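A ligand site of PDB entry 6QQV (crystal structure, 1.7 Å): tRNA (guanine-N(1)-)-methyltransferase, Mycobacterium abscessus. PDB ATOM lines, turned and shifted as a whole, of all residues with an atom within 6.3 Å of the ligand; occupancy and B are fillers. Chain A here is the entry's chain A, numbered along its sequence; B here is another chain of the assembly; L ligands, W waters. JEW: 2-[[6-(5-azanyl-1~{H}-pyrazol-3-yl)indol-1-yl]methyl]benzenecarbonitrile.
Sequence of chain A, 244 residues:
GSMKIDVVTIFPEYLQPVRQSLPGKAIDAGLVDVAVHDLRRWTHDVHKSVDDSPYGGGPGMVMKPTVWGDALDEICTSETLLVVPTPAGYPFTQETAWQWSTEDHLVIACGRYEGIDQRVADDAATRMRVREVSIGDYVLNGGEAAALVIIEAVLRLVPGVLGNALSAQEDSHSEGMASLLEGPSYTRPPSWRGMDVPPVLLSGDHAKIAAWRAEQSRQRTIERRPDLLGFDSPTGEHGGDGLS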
ATOM      1  N   PRO A  85       7.077  -1.031  19.308  1.00  0.00           N
ATOM      2  CA  PRO A  85       8.494  -1.263  19.578  1.00  0.00           C
ATOM      3  C   PRO A  85       9.305   0.014  19.511  1.00  0.00           C
ATOM      4  O   PRO A  85       9.055   0.868  18.674  1.00  0.00           O
ATOM      5  CB  PRO A  85       8.891  -2.247  18.469  1.00  0.00           C
ATOM      6  CG  PRO A  85       7.643  -3.021  18.210  1.00  0.00           C
ATOM      7  CD  PRO A  85       6.549  -1.940  18.269  1.00  0.00           C
ATOM      8  N   THR A  86      10.279   0.133  20.406  1.00  0.00           N
ATOM      9  CA  THR A  86      11.165   1.304  20.400  1.00  0.00           C
ATOM     10  C   THR A  86      12.331   0.999  21.328  1.00  0.00           C
ATOM     11  O   THR A  86      12.136   0.350  22.357  1.00  0.00           O
ATOM     12  CB  THR A  86      10.446   2.609  20.857  1.00  0.00           C
ATOM     13  OG1 THR A  86      11.425   3.620  21.190  1.00  0.00           O
ATOM     14  CG2 THR A  86       9.501   2.381  22.039  1.00  0.00           C
ATOM     15  N   PRO A  87      13.530   1.464  20.964  1.00  0.00           N
ATOM     16  CA  PRO A  87      14.700   1.267  21.846  1.00  0.00           C
ATOM     17  C   PRO A  87      14.513   1.913  23.206  1.00  0.00           C
ATOM     18  O   PRO A  87      15.190   1.538  24.170  1.00  0.00           O
ATOM     19  CB  PRO A  87      15.850   1.960  21.094  1.00  0.00           C
ATOM     20  CG  PRO A  87      15.362   2.207  19.727  1.00  0.00           C
ATOM     21  CD  PRO A  87      13.857   2.240  19.762  1.00  0.00           C
ATOM     22  N   ALA A  88      13.612   2.896  23.277  1.00  0.00           N
ATOM     23  CA  ALA A  88      13.365   3.628  24.513  1.00  0.00           C
ATOM     24  C   ALA A  88      12.165   3.078  25.270  1.00  0.00           C
ATOM     25  O   ALA A  88      11.652   3.733  26.178  1.00  0.00           O
ATOM     26  CB  ALA A  88      13.155   5.122  24.208  1.00  0.00           C
ATOM     27  N   CYS A 110       4.962  -0.765  13.708  1.00  0.00           N
ATOM     28  CA  CYS A 110       6.396  -0.811  13.437  1.00  0.00           C
ATOM     29  C   CYS A 110       6.907   0.473  12.847  1.00  0.00           C
ATOM     30  O   CYS A 110       6.499   0.879  11.746  1.00  0.00           O
ATOM     31  CB  CYS A 110       6.730  -1.959  12.479  1.00  0.00           C
ATOM     32  SG  CYS A 110       6.238  -3.575  13.044  1.00  0.00           S
ATOM     33  N   GLY A 111       7.816   1.132  13.555  1.00  0.00           N
ATOM     34  CA  GLY A 111       8.413   2.348  13.063  1.00  0.00           C
ATOM     35  C   GLY A 111       9.637   2.075  12.210  1.00  0.00           C
ATOM     36  O   GLY A 111      10.165   0.961  12.185  1.00  0.00           O
ATOM     37  N   ARG A 112      10.087   3.119  11.519  1.00  0.00           N
ATOM     38  CA  ARG A 112      11.355   3.120  10.805  1.00  0.00           C
ATOM     39  C   ARG A 112      11.969   4.491  11.017  1.00  0.00           C
ATOM     40  O   ARG A 112      11.487   5.256  11.861  1.00  0.00           O
ATOM     41  CB  ARG A 112      11.184   2.786   9.328  1.00  0.00           C
ATOM     42  CG  ARG A 112      11.050   1.294   9.049  1.00  0.00           C
ATOM     43  CD  ARG A 112      12.424   0.661   8.856  1.00  0.00           C
ATOM     44  NE  ARG A 112      12.393  -0.766   9.114  1.00  0.00           N
ATOM     45  CZ  ARG A 112      13.378  -1.600   8.823  1.00  0.00           C
ATOM     46  NH1 ARG A 112      14.489  -1.132   8.251  1.00  0.00           N
ATOM     47  NH2 ARG A 112      13.278  -2.889   9.108  1.00  0.00           N
ATOM     48  N   TYR A 113      13.032   4.806  10.276  1.00  0.00           N
ATOM     49  CA  TYR A 113      13.715   6.092  10.449  1.00  0.00           C
ATOM     50  C   TYR A 113      14.146   6.251  11.903  1.00  0.00           C
ATOM     51  O   TYR A 113      14.753   5.332  12.465  1.00  0.00           O
ATOM     52  CB  TYR A 113      12.806   7.240   9.985  1.00  0.00           C
ATOM     53  CG  TYR A 113      12.301   7.052   8.565  1.00  0.00           C
ATOM     54  CD1 TYR A 113      13.047   7.493   7.475  1.00  0.00           C
ATOM     55  CD2 TYR A 113      11.093   6.402   8.321  1.00  0.00           C
ATOM     56  CE1 TYR A 113      12.600   7.288   6.177  1.00  0.00           C
ATOM     57  CE2 TYR A 113      10.640   6.193   7.029  1.00  0.00           C
ATOM     58  CZ  TYR A 113      11.392   6.641   5.968  1.00  0.00           C
ATOM     59  OH  TYR A 113      10.937   6.450   4.686  1.00  0.00           O
ATOM     60  N   GLU A 114      13.838   7.381  12.514  1.00  0.00           N
ATOM     61  CA  GLU A 114      14.228   7.612  13.915  1.00  0.00           C
ATOM     62  C   GLU A 114      13.081   7.440  14.893  1.00  0.00           C
ATOM     63  O   GLU A 114      13.192   7.809  16.055  1.00  0.00           O
ATOM     64  CB  GLU A 114      14.831   8.999  14.097  1.00  0.00           C
ATOM     65  CG  GLU A 114      16.081   9.249  13.289  1.00  0.00           C
ATOM     66  CD  GLU A 114      17.318   8.632  13.928  1.00  0.00           C
ATOM     67  OE1 GLU A 114      17.733   7.547  13.484  1.00  0.00           O
ATOM     68  OE2 GLU A 114      17.857   9.243  14.881  1.00  0.00           O
ATOM     69  N   GLY A 115      11.969   6.858  14.432  1.00  0.00           N
ATOM     70  CA  GLY A 115      10.847   6.588  15.303  1.00  0.00           C
ATOM     71  C   GLY A 115       9.588   7.315  14.891  1.00  0.00           C
ATOM     72  O   GLY A 115       9.563   7.941  13.834  1.00  0.00           O
ATOM     73  N   ILE A 116       8.563   7.248  15.733  1.00  0.00           N
ATOM     74  CA  ILE A 116       7.254   7.799  15.415  1.00  0.00           C
ATOM     75  C   ILE A 116       6.978   9.021  16.277  1.00  0.00           C
ATOM     76  O   ILE A 116       7.281   9.011  17.473  1.00  0.00           O
ATOM     77  CB  ILE A 116       6.144   6.748  15.629  1.00  0.00           C
ATOM     78  CG1 ILE A 116       6.482   5.473  14.852  1.00  0.00           C
ATOM     79  CG2 ILE A 116       4.751   7.329  15.281  1.00  0.00           C
ATOM     80  CD1 ILE A 116       5.550   4.301  15.156  1.00  0.00           C
ATOM     81  N   VAL A 133       7.634  -0.683  23.938  1.00  0.00           N
ATOM     82  CA  VAL A 133       8.501  -1.722  24.484  1.00  0.00           C
ATOM     83  C   VAL A 133       9.792  -1.891  23.707  1.00  0.00           C
ATOM     84  O   VAL A 133       9.823  -1.733  22.488  1.00  0.00           O
ATOM     85  CB  VAL A 133       7.786  -3.114  24.550  1.00  0.00           C
ATOM     86  CG1 VAL A 133       6.674  -3.115  25.602  1.00  0.00           C
ATOM     87  CG2 VAL A 133       7.245  -3.525  23.187  1.00  0.00           C
ATOM     88  N   SER A 134      10.839  -2.261  24.441  1.00  0.00           N
ATOM     89  CA  SER A 134      12.138  -2.623  23.880  1.00  0.00           C
ATOM     90  C   SER A 134      12.357  -4.122  24.035  1.00  0.00           C
ATOM     91  O   SER A 134      12.027  -4.678  25.074  1.00  0.00           O
ATOM     92  CB  SER A 134      13.257  -1.841  24.582  1.00  0.00           C
ATOM     93  OG  SER A 134      14.540  -2.332  24.244  1.00  0.00           O
ATOM     94  N   ILE A 135      12.938  -4.778  23.021  1.00  0.00           N
ATOM     95  CA  ILE A 135      13.178  -6.226  23.152  1.00  0.00           C
ATOM     96  C   ILE A 135      14.591  -6.582  23.599  1.00  0.00           C
ATOM     97  O   ILE A 135      14.920  -7.757  23.758  1.00  0.00           O
ATOM     98  CB  ILE A 135      12.913  -6.993  21.844  1.00  0.00           C
ATOM     99  CG1 ILE A 135      13.804  -6.485  20.709  1.00  0.00           C
ATOM    100  CG2 ILE A 135      11.427  -6.906  21.467  1.00  0.00           C
ATOM    101  CD1 ILE A 135      13.912  -7.515  19.535  1.00  0.00           C
ATOM    102  N   GLY A 136      15.414  -5.563  23.801  1.00  0.00           N
ATOM    103  CA  GLY A 136      16.780  -5.785  24.246  1.00  0.00           C
ATOM    104  C   GLY A 136      17.614  -4.541  24.100  1.00  0.00           C
ATOM    105  O   GLY A 136      17.218  -3.580  23.430  1.00  0.00           O
ATOM    106  N   ASP A 137      18.797  -4.561  24.697  1.00  0.00           N
ATOM    107  CA  ASP A 137      19.607  -3.349  24.723  1.00  0.00           C
ATOM    108  C   ASP A 137      20.537  -3.215  23.522  1.00  0.00           C
ATOM    109  O   ASP A 137      21.752  -3.176  23.660  1.00  0.00           O
ATOM    110  CB  ASP A 137      20.405  -3.290  26.029  1.00  0.00           C
ATOM    111  CG  ASP A 137      19.517  -3.072  27.234  1.00  0.00           C
ATOM    112  OD1 ASP A 137      18.366  -2.639  27.035  1.00  0.00           O
ATOM    113  OD2 ASP A 137      19.974  -3.318  28.369  1.00  0.00           O
ATOM    114  N   TYR A 138      19.915  -3.131  22.349  1.00  0.00           N
ATOM    115  CA  TYR A 138      20.616  -2.913  21.092  1.00  0.00           C
ATOM    116  C   TYR A 138      19.638  -2.126  20.232  1.00  0.00           C
ATOM    117  O   TYR A 138      18.460  -2.061  20.548  1.00  0.00           O
ATOM    118  CB  TYR A 138      20.999  -4.226  20.411  1.00  0.00           C
ATOM    119  CG  TYR A 138      19.928  -5.255  20.616  1.00  0.00           C
ATOM    120  CD1 TYR A 138      18.743  -5.223  19.855  1.00  0.00           C
ATOM    121  CD2 TYR A 138      20.052  -6.244  21.579  1.00  0.00           C
ATOM    122  CE1 TYR A 138      17.733  -6.130  20.063  1.00  0.00           C
ATOM    123  CE2 TYR A 138      19.046  -7.176  21.790  1.00  0.00           C
ATOM    124  CZ  TYR A 138      17.892  -7.111  21.019  1.00  0.00           C
ATOM    125  OH  TYR A 138      16.880  -8.012  21.215  1.00  0.00           O
ATOM    126  N   VAL A 139      20.157  -1.548  19.157  1.00  0.00           N
ATOM    127  CA  VAL A 139      19.369  -0.702  18.258  1.00  0.00           C
ATOM    128  C   VAL A 139      19.165  -1.395  16.934  1.00  0.00           C
ATOM    129  O   VAL A 139      20.129  -1.839  16.302  1.00  0.00           O
ATOM    130  CB  VAL A 139      20.069   0.654  18.028  1.00  0.00           C
ATOM    131  CG1 VAL A 139      19.234   1.519  17.064  1.00  0.00           C
ATOM    132  CG2 VAL A 139      20.264   1.365  19.338  1.00  0.00           C
ATOM    133  N   LEU A 140      17.912  -1.497  16.514  1.00  0.00           N
ATOM    134  CA  LEU A 140      17.561  -2.061  15.215  1.00  0.00           C
ATOM    135  C   LEU A 140      17.329  -0.934  14.211  1.00  0.00           C
ATOM    136  O   LEU A 140      17.361   0.247  14.565  1.00  0.00           O
ATOM    137  CB  LEU A 140      16.304  -2.918  15.343  1.00  0.00           C
ATOM    138  CG  LEU A 140      16.349  -4.087  16.338  1.00  0.00           C
ATOM    139  CD1 LEU A 140      14.952  -4.580  16.628  1.00  0.00           C
ATOM    140  CD2 LEU A 140      17.217  -5.217  15.790  1.00  0.00           C
ATOM    141  N   ASN A 141      17.090  -1.286  12.952  1.00  0.00           N
ATOM    142  CA  ASN A 141      16.746  -0.267  11.950  1.00  0.00           C
ATOM    143  C   ASN A 141      15.280   0.138  12.034  1.00  0.00           C
ATOM    144  O   ASN A 141      14.877   1.197  11.534  1.00  0.00           O
ATOM    145  CB  ASN A 141      17.039  -0.769  10.543  1.00  0.00           C
ATOM    146  CG  ASN A 141      18.505  -0.760  10.202  1.00  0.00           C
ATOM    147  OD1 ASN A 141      19.213   0.197  10.530  1.00  0.00           O
ATOM    148  ND2 ASN A 141      18.964  -1.809   9.545  1.00  0.00           N
ATOM    149  N   GLY A 142      14.462  -0.709  12.644  1.00  0.00           N
ATOM    150  CA  GLY A 142      13.036  -0.428  12.710  1.00  0.00           C
ATOM    151  C   GLY A 142      12.326  -1.468  13.558  1.00  0.00           C
ATOM    152  O   GLY A 142      12.970  -2.348  14.122  1.00  0.00           O
ATOM    153  N   GLY A 143      11.013  -1.368  13.641  1.00  0.00           N
ATOM    154  CA  GLY A 143      10.232  -2.196  14.550  1.00  0.00           C
ATOM    155  C   GLY A 143       9.951  -3.612  14.086  1.00  0.00           C
ATOM    156  O   GLY A 143       9.479  -4.430  14.883  1.00  0.00           O
ATOM    157  N   GLU A 144      10.243  -3.921  12.828  1.00  0.00           N
ATOM    158  CA  GLU A 144       9.781  -5.199  12.267  1.00  0.00           C
ATOM    159  C   GLU A 144      10.443  -6.422  12.906  1.00  0.00           C
ATOM    160  O   GLU A 144       9.761  -7.405  13.196  1.00  0.00           O
ATOM    161  CB  GLU A 144      10.008  -5.228  10.750  1.00  0.00           C
ATOM    162  CG  GLU A 144       9.096  -4.290   9.966  1.00  0.00           C
ATOM    163  CD  GLU A 144       9.541  -2.835   9.993  1.00  0.00           C
ATOM    164  OE1 GLU A 144      10.656  -2.521  10.458  1.00  0.00           O
ATOM    165  OE2 GLU A 144       8.774  -1.973   9.515  1.00  0.00           O
ATOM    166  N   ALA A 146      11.575  -6.609  15.866  1.00  0.00           N
ATOM    167  CA  ALA A 146      10.994  -6.651  17.207  1.00  0.00           C
ATOM    168  C   ALA A 146       9.602  -7.260  17.155  1.00  0.00           C
ATOM    169  O   ALA A 146       9.228  -8.048  18.022  1.00  0.00           O
ATOM    170  CB  ALA A 146      10.942  -5.262  17.826  1.00  0.00           C
ATOM    171  N   ARG B 156      24.105  -2.529  10.694  1.00  0.00           N
ATOM    172  CA  ARG B 156      23.933  -1.085  10.626  1.00  0.00           C
ATOM    173  C   ARG B 156      25.139  -0.334  11.219  1.00  0.00           C
ATOM    174  O   ARG B 156      25.262   0.887  11.079  1.00  0.00           O
ATOM    175  CB  ARG B 156      22.637  -0.656  11.313  1.00  0.00           C
ATOM    176  CG  ARG B 156      22.512  -1.042  12.766  1.00  0.00           C
ATOM    177  CD  ARG B 156      21.092  -0.791  13.271  1.00  0.00           C
ATOM    178  NE  ARG B 156      20.738   0.626  13.209  1.00  0.00           N
ATOM    179  CZ  ARG B 156      21.196   1.562  14.044  1.00  0.00           C
ATOM    180  NH1 ARG B 156      22.065   1.249  15.003  1.00  0.00           N
ATOM    181  NH2 ARG B 156      20.786   2.811  13.919  1.00  0.00           N
ATOM    182  N   GLU B 182      16.523   7.317  24.437  1.00  0.00           N
ATOM    183  CA  GLU B 182      16.175   8.457  23.625  1.00  0.00           C
ATOM    184  C   GLU B 182      14.835   9.031  24.090  1.00  0.00           C
ATOM    185  O   GLU B 182      13.936   8.280  24.454  1.00  0.00           O
ATOM    186  CB  GLU B 182      16.098   8.070  22.140  1.00  0.00           C
ATOM    187  CG  GLU B 182      16.713   9.100  21.208  1.00  0.00           C
ATOM    188  CD  GLU B 182      18.216   9.238  21.399  1.00  0.00           C
ATOM    189  OE1 GLU B 182      18.931   8.246  21.142  1.00  0.00           O
ATOM    190  OE2 GLU B 182      18.671  10.326  21.805  1.00  0.00           O
HETATM  191  C13 JEW L   1      13.560  -0.230  17.392  1.00  0.00           C
HETATM  192  C15 JEW L   1      11.500   0.545  16.418  1.00  0.00           C
HETATM  193  C17 JEW L   1      11.884   2.444  14.648  1.00  0.00           C
HETATM  194  C20 JEW L   1      13.806  -1.706  19.494  1.00  0.00           C
HETATM  195  C21 JEW L   1      14.903  -2.289  20.145  1.00  0.00           C
HETATM  196  N01 JEW L   1      12.681   4.188  17.220  1.00  0.00           N
HETATM  197  C02 JEW L   1      13.775   4.367  16.946  1.00  0.00           C
HETATM  198  C03 JEW L   1      15.236   4.610  16.621  1.00  0.00           C
HETATM  199  C04 JEW L   1      15.955   3.939  15.623  1.00  0.00           C
HETATM  200  C05 JEW L   1      17.294   4.265  15.409  1.00  0.00           C
HETATM  201  C06 JEW L   1      17.909   5.239  16.172  1.00  0.00           C
HETATM  202  C07 JEW L   1      17.198   5.896  17.154  1.00  0.00           C
HETATM  203  C08 JEW L   1      15.872   5.581  17.373  1.00  0.00           C
HETATM  204  C09 JEW L   1      15.437   2.856  14.689  1.00  0.00           C
HETATM  205  N10 JEW L   1      14.057   2.503  14.861  1.00  0.00           N
HETATM  206  C11 JEW L   1      13.611   1.530  15.731  1.00  0.00           C
HETATM  207  C12 JEW L   1      14.299   0.678  16.638  1.00  0.00           C
HETATM  208  C14 JEW L   1      12.165  -0.299  17.308  1.00  0.00           C
HETATM  209  C16 JEW L   1      12.237   1.458  15.635  1.00  0.00           C
HETATM  210  C18 JEW L   1      13.044   3.052  14.206  1.00  0.00           C
HETATM  211  C19 JEW L   1      14.306  -1.064  18.384  1.00  0.00           C
HETATM  212  N22 JEW L   1      16.000  -1.953  19.436  1.00  0.00           N
HETATM  213  N23 JEW L   1      15.634  -1.193  18.374  1.00  0.00           N
HETATM  214  N24 JEW L   1      14.899  -3.081  21.323  1.00  0.00           N
HETATM  215  O   HOH W   1       9.670   3.534  17.134  1.00  0.00           O
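The backbone carbonyl oxygen (O) of Gly 136 lies within hydrogen-bond range of a nitrogen (N24) of the ligand. N of Leu 140 is in hydrogen-bond range of N23 of the ligand (3.0 Å). OG of Ser 134 is in hydrogen-bond range of N24 of the ligand, at 3.0 Å. O of Tyr 138 sits at hydrogen-bond distance from N22 of the ligand.
The side-chain hydroxyl (OH) of Tyr 138 is in hydrogen-bond range of the backbone carbonyl oxygen (O) of Ile 135 (3.2 Å). The backbone carbonyl oxygen of Gly 136 sits at hydrogen-bond distance from the side-chain hydroxyl of Ser 134, 3.1 Å away. The guanidinium group of Arg 156 of chain B sits at hydrogen-bond distance from the side-chain amide oxygen of Asn 141 (3.1 Å). The backbone carbonyl oxygen of Gly 111 lies within hydrogen-bond range of the backbone NH of Gly 143, at 2.9 Å. The side-chain hydroxyl (OG1) of Thr 86 sits close to the backbone NH (N) of Ala 88, 3.1 Å away. The guanidinium group of Arg 112 is in salt-bridge range of the side-chain carboxylate of Glu 144 (2.8 Å). The backbone NH (N) of Thr 86 sits at hydrogen-bond distance from the backbone carbonyl oxygen (O) of Val 133 (2.8 Å).
A nitrogen (N24) of the ligand lies close to the backbone NH (N) of Ile 135, at 3.1 Å. Pro 85 touches the ligand. Thr 86 touches the ligand (C to C20, 3.6 Å). Pro 87 touches the ligand (CD to N01, 3.4 Å). C of Gly 111 touches C17 of the ligand (3.3 Å). Arg 112 touches the ligand (O to C18, 3.6 Å). Tyr 113 touches the ligand (O to C18, 3.3 Å). Glu 114 touches the ligand. Gly 115 touches the ligand (CA to N01, 3.6 Å). Val 139 touches the ligand. Asn 141 touches the ligand (O to C09, 3.6 Å). Gly 142 touches the ligand (CA to C16, 3.6 Å). Gly 143 touches the ligand. Hydrophobic or aromatic side chains within 4 Å of the ligand: Pro 85, Pro 87, Ile 135, Val 139 and Leu 140. Within 4 Å of the ligand: Pro 85, Thr 86, Pro 87, Gly 111, Arg 112, Tyr 113, Glu 114, Gly 115, Ser 134, Ile 135, Gly 136, Tyr 138, Val 139, Leu 140, Asn 141, Gly 142 and Gly 143.
Water W1 lies within hydrogen-bond range of N01 of the ligand (3.1 Å) and O of Pro 85 (3.1 Å).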
